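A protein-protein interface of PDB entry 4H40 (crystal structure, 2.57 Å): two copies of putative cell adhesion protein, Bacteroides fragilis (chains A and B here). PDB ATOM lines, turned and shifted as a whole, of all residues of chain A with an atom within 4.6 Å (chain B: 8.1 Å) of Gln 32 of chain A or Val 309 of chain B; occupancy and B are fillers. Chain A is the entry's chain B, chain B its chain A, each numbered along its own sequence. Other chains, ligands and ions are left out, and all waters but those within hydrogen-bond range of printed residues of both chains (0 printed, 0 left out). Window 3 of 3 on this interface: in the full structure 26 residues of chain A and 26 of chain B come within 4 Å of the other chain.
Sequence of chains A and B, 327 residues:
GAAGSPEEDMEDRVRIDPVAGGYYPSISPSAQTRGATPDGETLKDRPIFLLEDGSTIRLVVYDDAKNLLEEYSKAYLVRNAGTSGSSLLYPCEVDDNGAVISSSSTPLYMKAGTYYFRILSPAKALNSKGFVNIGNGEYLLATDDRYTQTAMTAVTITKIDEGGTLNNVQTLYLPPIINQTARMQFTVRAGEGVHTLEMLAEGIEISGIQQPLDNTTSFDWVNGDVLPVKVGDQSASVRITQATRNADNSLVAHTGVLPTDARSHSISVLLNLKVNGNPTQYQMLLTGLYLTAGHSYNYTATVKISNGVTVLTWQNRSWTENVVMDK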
ATOM      1  N   SER A  30     -21.948 -31.561 -10.492  1.00  0.00           N
ATOM      2  CA  SER A  30     -23.375 -31.601 -10.798  1.00  0.00           C
ATOM      3  C   SER A  30     -24.016 -30.672  -9.773  1.00  0.00           C
ATOM      4  O   SER A  30     -23.572 -30.663  -8.610  1.00  0.00           O
ATOM      5  CB  SER A  30     -23.930 -33.028 -10.746  1.00  0.00           C
ATOM      6  OG  SER A  30     -23.851 -33.609  -9.454  1.00  0.00           O
ATOM      7  N   ALA A  31     -24.996 -29.844 -10.215  1.00  0.00           N
ATOM      8  CA  ALA A  31     -25.693 -28.824  -9.416  1.00  0.00           C
ATOM      9  C   ALA A  31     -25.974 -29.243  -7.955  1.00  0.00           C
ATOM     10  O   ALA A  31     -26.638 -30.255  -7.689  1.00  0.00           O
ATOM     11  CB  ALA A  31     -26.975 -28.420 -10.090  1.00  0.00           C
ATOM     12  N   GLN A  32     -25.420 -28.438  -7.026  1.00  0.00           N
ATOM     13  CA  GLN A  32     -25.435 -28.603  -5.572  1.00  0.00           C
ATOM     14  C   GLN A  32     -26.835 -28.534  -4.940  1.00  0.00           C
ATOM     15  O   GLN A  32     -27.738 -27.888  -5.479  1.00  0.00           O
ATOM     16  CB  GLN A  32     -24.559 -27.516  -4.926  1.00  0.00           C
ATOM     17  CG  GLN A  32     -23.054 -27.772  -5.000  1.00  0.00           C
ATOM     18  CD  GLN A  32     -22.241 -26.782  -4.186  1.00  0.00           C
ATOM     19  OE1 GLN A  32     -22.773 -25.955  -3.426  1.00  0.00           O
ATOM     20  NE2 GLN A  32     -20.919 -26.861  -4.312  1.00  0.00           N
ATOM     21  N   THR A  33     -26.984 -29.195  -3.768  1.00  0.00           N
ATOM     22  CA  THR A  33     -28.197 -29.177  -2.953  1.00  0.00           C
ATOM     23  C   THR A  33     -28.099 -27.884  -2.131  1.00  0.00           C
ATOM     24  O   THR A  33     -27.296 -27.795  -1.193  1.00  0.00           O
ATOM     25  CB  THR A  33     -28.330 -30.483  -2.125  1.00  0.00           C
ATOM     26  OG1 THR A  33     -28.447 -31.597  -3.018  1.00  0.00           O
ATOM     27  CG2 THR A  33     -29.522 -30.460  -1.153  1.00  0.00           C
ATOM     28  N   ARG A  34     -28.869 -26.861  -2.542  1.00  0.00           N
ATOM     29  CA  ARG A  34     -28.888 -25.531  -1.927  1.00  0.00           C
ATOM     30  C   ARG A  34     -29.727 -25.509  -0.625  1.00  0.00           C
ATOM     31  O   ARG A  34     -30.127 -24.435  -0.156  1.00  0.00           O
ATOM     32  CB  ARG A  34     -29.428 -24.508  -2.947  1.00  0.00           C
ATOM     33  N   THR A 292     -14.401 -26.964  -6.280  1.00  0.00           N
ATOM     34  CA  THR A 292     -14.860 -27.162  -4.901  1.00  0.00           C
ATOM     35  C   THR A 292     -14.384 -28.527  -4.344  1.00  0.00           C
ATOM     36  O   THR A 292     -14.004 -29.423  -5.105  1.00  0.00           O
ATOM     37  CB  THR A 292     -16.386 -26.998  -4.796  1.00  0.00           C
ATOM     38  OG1 THR A 292     -17.045 -27.894  -5.690  1.00  0.00           O
ATOM     39  CG2 THR A 292     -16.836 -25.618  -5.135  1.00  0.00           C
ATOM     40  N   GLU A 321     -24.698 -22.912 -13.571  1.00  0.00           N
ATOM     41  CA  GLU A 321     -25.981 -22.660 -12.914  1.00  0.00           C
ATOM     42  C   GLU A 321     -26.680 -21.450 -13.483  1.00  0.00           C
ATOM     43  O   GLU A 321     -26.060 -20.652 -14.182  1.00  0.00           O
ATOM     44  CB  GLU A 321     -25.788 -22.494 -11.396  1.00  0.00           C
ATOM     45  CG  GLU A 321     -25.490 -23.808 -10.682  1.00  0.00           C
ATOM     46  CD  GLU A 321     -25.576 -23.824  -9.166  1.00  0.00           C
ATOM     47  OE1 GLU A 321     -26.254 -22.943  -8.582  1.00  0.00           O
ATOM     48  OE2 GLU A 321     -24.985 -24.749  -8.563  1.00  0.00           O
ATOM     49  N   GLU B 192     -33.459 -33.828 -18.285  1.00  0.00           N
ATOM     50  CA  GLU B 192     -34.261 -34.337 -17.176  1.00  0.00           C
ATOM     51  C   GLU B 192     -35.026 -33.215 -16.435  1.00  0.00           C
ATOM     52  O   GLU B 192     -34.416 -32.283 -15.895  1.00  0.00           O
ATOM     53  CB  GLU B 192     -33.411 -35.168 -16.183  1.00  0.00           C
ATOM     54  N   TYR B 282     -27.831 -18.433 -18.683  1.00  0.00           N
ATOM     55  CA  TYR B 282     -26.644 -19.265 -18.531  1.00  0.00           C
ATOM     56  C   TYR B 282     -25.502 -18.698 -19.310  1.00  0.00           C
ATOM     57  O   TYR B 282     -25.700 -18.228 -20.436  1.00  0.00           O
ATOM     58  CB  TYR B 282     -26.908 -20.681 -19.036  1.00  0.00           C
ATOM     59  CG  TYR B 282     -28.137 -21.313 -18.444  1.00  0.00           C
ATOM     60  CD1 TYR B 282     -28.111 -21.880 -17.166  1.00  0.00           C
ATOM     61  CD2 TYR B 282     -29.324 -21.376 -19.167  1.00  0.00           C
ATOM     62  CE1 TYR B 282     -29.241 -22.484 -16.622  1.00  0.00           C
ATOM     63  CE2 TYR B 282     -30.461 -21.966 -18.628  1.00  0.00           C
ATOM     64  CZ  TYR B 282     -30.417 -22.511 -17.352  1.00  0.00           C
ATOM     65  OH  TYR B 282     -31.527 -23.119 -16.821  1.00  0.00           O
ATOM     66  N   VAL B 303     -30.174 -28.560 -20.903  1.00  0.00           N
ATOM     67  CA  VAL B 303     -30.758 -27.948 -19.709  1.00  0.00           C
ATOM     68  C   VAL B 303     -31.298 -29.102 -18.834  1.00  0.00           C
ATOM     69  O   VAL B 303     -32.141 -29.878 -19.281  1.00  0.00           O
ATOM     70  CB  VAL B 303     -31.826 -26.880 -20.037  1.00  0.00           C
ATOM     71  CG1 VAL B 303     -32.325 -26.206 -18.769  1.00  0.00           C
ATOM     72  CG2 VAL B 303     -31.264 -25.836 -20.979  1.00  0.00           C
ATOM     73  N   LYS B 304     -30.773 -29.231 -17.615  1.00  0.00           N
ATOM     74  CA  LYS B 304     -31.151 -30.277 -16.658  1.00  0.00           C
ATOM     75  C   LYS B 304     -31.694 -29.703 -15.370  1.00  0.00           C
ATOM     76  O   LYS B 304     -31.316 -28.595 -15.002  1.00  0.00           O
ATOM     77  CB  LYS B 304     -29.905 -31.118 -16.301  1.00  0.00           C
ATOM     78  CG  LYS B 304     -29.566 -32.222 -17.286  1.00  0.00           C
ATOM     79  CD  LYS B 304     -28.219 -32.857 -16.960  1.00  0.00           C
ATOM     80  CE  LYS B 304     -27.731 -33.720 -18.102  1.00  0.00           C
ATOM     81  NZ  LYS B 304     -26.283 -34.066 -17.979  1.00  0.00           N
ATOM     82  N   ILE B 305     -32.525 -30.480 -14.655  1.00  0.00           N
ATOM     83  CA  ILE B 305     -32.982 -30.179 -13.288  1.00  0.00           C
ATOM     84  C   ILE B 305     -32.272 -31.201 -12.392  1.00  0.00           C
ATOM     85  O   ILE B 305     -32.541 -32.401 -12.531  1.00  0.00           O
ATOM     86  CB  ILE B 305     -34.521 -30.182 -13.067  1.00  0.00           C
ATOM     87  CG1 ILE B 305     -35.329 -29.450 -14.172  1.00  0.00           C
ATOM     88  CG2 ILE B 305     -34.878 -29.722 -11.659  1.00  0.00           C
ATOM     89  CD1 ILE B 305     -35.195 -27.945 -14.315  1.00  0.00           C
ATOM     90  N   SER B 306     -31.335 -30.747 -11.520  1.00  0.00           N
ATOM     91  CA  SER B 306     -30.578 -31.644 -10.631  1.00  0.00           C
ATOM     92  C   SER B 306     -31.392 -32.007  -9.387  1.00  0.00           C
ATOM     93  O   SER B 306     -31.465 -33.184  -9.017  1.00  0.00           O
ATOM     94  CB  SER B 306     -29.242 -31.028 -10.235  1.00  0.00           C
ATOM     95  OG  SER B 306     -28.271 -31.254 -11.247  1.00  0.00           O
ATOM     96  N   ASN B 307     -31.992 -30.995  -8.739  1.00  0.00           N
ATOM     97  CA  ASN B 307     -32.881 -31.171  -7.594  1.00  0.00           C
ATOM     98  C   ASN B 307     -34.109 -30.308  -7.872  1.00  0.00           C
ATOM     99  O   ASN B 307     -35.140 -30.815  -8.319  1.00  0.00           O
ATOM    100  CB  ASN B 307     -32.196 -30.811  -6.262  1.00  0.00           C
ATOM    101  CG  ASN B 307     -30.776 -31.271  -6.112  1.00  0.00           C
ATOM    102  OD1 ASN B 307     -30.501 -32.317  -5.517  1.00  0.00           O
ATOM    103  ND2 ASN B 307     -29.830 -30.466  -6.588  1.00  0.00           N
ATOM    104  N   GLY B 308     -33.945 -29.007  -7.673  1.00  0.00           N
ATOM    105  CA  GLY B 308     -34.923 -27.971  -7.962  1.00  0.00           C
ATOM    106  C   GLY B 308     -34.212 -26.949  -8.816  1.00  0.00           C
ATOM    107  O   GLY B 308     -34.840 -26.160  -9.529  1.00  0.00           O
ATOM    108  N   VAL B 309     -32.869 -27.017  -8.762  1.00  0.00           N
ATOM    109  CA  VAL B 309     -31.900 -26.180  -9.461  1.00  0.00           C
ATOM    110  C   VAL B 309     -31.787 -26.597 -10.944  1.00  0.00           C
ATOM    111  O   VAL B 309     -31.702 -27.785 -11.270  1.00  0.00           O
ATOM    112  CB  VAL B 309     -30.527 -26.228  -8.718  1.00  0.00           C
ATOM    113  CG1 VAL B 309     -29.972 -27.648  -8.623  1.00  0.00           C
ATOM    114  CG2 VAL B 309     -29.506 -25.268  -9.327  1.00  0.00           C
ATOM    115  N   THR B 310     -31.805 -25.596 -11.831  1.00  0.00           N
ATOM    116  CA  THR B 310     -31.668 -25.805 -13.275  1.00  0.00           C
ATOM    117  C   THR B 310     -30.209 -25.545 -13.661  1.00  0.00           C
ATOM    118  O   THR B 310     -29.650 -24.524 -13.248  1.00  0.00           O
ATOM    119  CB  THR B 310     -32.649 -24.913 -14.079  1.00  0.00           C
ATOM    120  OG1 THR B 310     -32.106 -23.594 -14.220  1.00  0.00           O
ATOM    121  CG2 THR B 310     -34.025 -24.823 -13.446  1.00  0.00           C
ATOM    122  N   VAL B 311     -29.593 -26.461 -14.431  1.00  0.00           N
ATOM    123  CA  VAL B 311     -28.212 -26.301 -14.914  1.00  0.00           C
ATOM    124  C   VAL B 311     -28.113 -26.502 -16.417  1.00  0.00           C
ATOM    125  O   VAL B 311     -28.960 -27.149 -17.026  1.00  0.00           O
ATOM    126  CB  VAL B 311     -27.159 -27.187 -14.206  1.00  0.00           C
ATOM    127  CG1 VAL B 311     -26.810 -26.619 -12.845  1.00  0.00           C
ATOM    128  CG2 VAL B 311     -27.575 -28.659 -14.124  1.00  0.00           C
ATOM    129  N   LEU B 312     -27.030 -25.976 -16.993  1.00  0.00           N
ATOM    130  CA  LEU B 312     -26.649 -26.107 -18.382  1.00  0.00           C
ATOM    131  C   LEU B 312     -25.321 -26.804 -18.426  1.00  0.00           C
ATOM    132  O   LEU B 312     -24.379 -26.407 -17.733  1.00  0.00           O
ATOM    133  CB  LEU B 312     -26.579 -24.757 -19.096  1.00  0.00           C
ATOM    134  CG  LEU B 312     -26.649 -24.854 -20.621  1.00  0.00           C
ATOM    135  CD1 LEU B 312     -28.033 -24.579 -21.109  1.00  0.00           C
ATOM    136  CD2 LEU B 312     -25.650 -23.906 -21.297  1.00  0.00           C
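Hydrophobic or aromatic side chains of chain A within 4 Å of the printed part of chain B: Ala 31.
Hydrophobic or aromatic side chains of chain B that line the printed part of chain A: Tyr 282, Val 309 and Val 311.
Along chain B the printed residues that touch a printed residue of chain A span positions 282 to 311.
Among the printed residues, 9 pairs touch across the chains.
Among the printed residues, no Asp or Glu carboxylate lies within 4 Å of a Lys or Arg side-chain nitrogen of the other chain.
OH of Tyr 282 of chain B sits at hydrogen-bond distance from OG1 of Thr 310 of chain B (2.7 Å).
O of Lys 304 of chain B lies within hydrogen-bond range of N of Val 311 of chain B, at 2.8 Å.
No position is printed for both chains.
Of the 9 pairs that touch across the chains among the printed residues, none has its exchanged pair printed and touching as well.
The backbone carbonyl oxygen of Ala 31 of chain A sits at hydrogen-bond distance from the side-chain amide nitrogen of Asn 307 of chain B, 3.4 Å away.
The side-chain amide oxygen (OD1) of Asn 307 of chain B lies within hydrogen-bond range of the side-chain hydroxyl (OG1) of Thr 33 of chain A, 3.3 Å away.
OG of Ser 306 of chain B touches CB of Ala 31 of chain A (3.3 Å).
Ala 31 of chain A touches Val 309 of chain B.
Ala 31 of chain A touches Val 311 of chain B (CB to CG1, 3.3 Å).
Asn 307 of chain B touches Gln 32 of chain A.
O of Gln 32 of chain A touches CG1 of Val 309 of chain B, 3.9 Å away.
Tyr 282 of chain B touches Glu 321 of chain A (CD1 to O, 3.8 Å).
Glu 321 of chain A touches Val 311 of chain B (CG to CG1, 3.8 Å).
Of chain B, only Ser 306 (3.3 Å), Asn 307 (3.4 Å), Val 309 (3.4 Å) and Val 311 (3.3 Å) come within 4 Å of Ala 31 of chain A.
Printed residues of chain B within 4 Å of Gln 32 of chain A: Asn 307 (3.5 Å) and Val 309 (3.9 Å).
Printed residues of chain B within 4 Å of Thr 33 of chain A: Asn 307 (3.3 Å).
Thr 292 of chain A touches none of the printed residues of chain B.
Lys 304 of chain B touches none of the printed residues of chain A.
Printed residues of chain A within 4 Å of Asn 307 of chain B: Ala 31, Gln 32 and Thr 33.
Printed residues of chain A within 4 Å of Val 311 of chain B: Ala 31 and Glu 321.
The nearest residue of chain A that does not touch Val 309 of chain B is Glu 321 of chain A (4.1 Å).
The nearest printed residue of chain A that does not touch Ser 306 of chain B is Ser 30 of chain A (4.5 Å).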
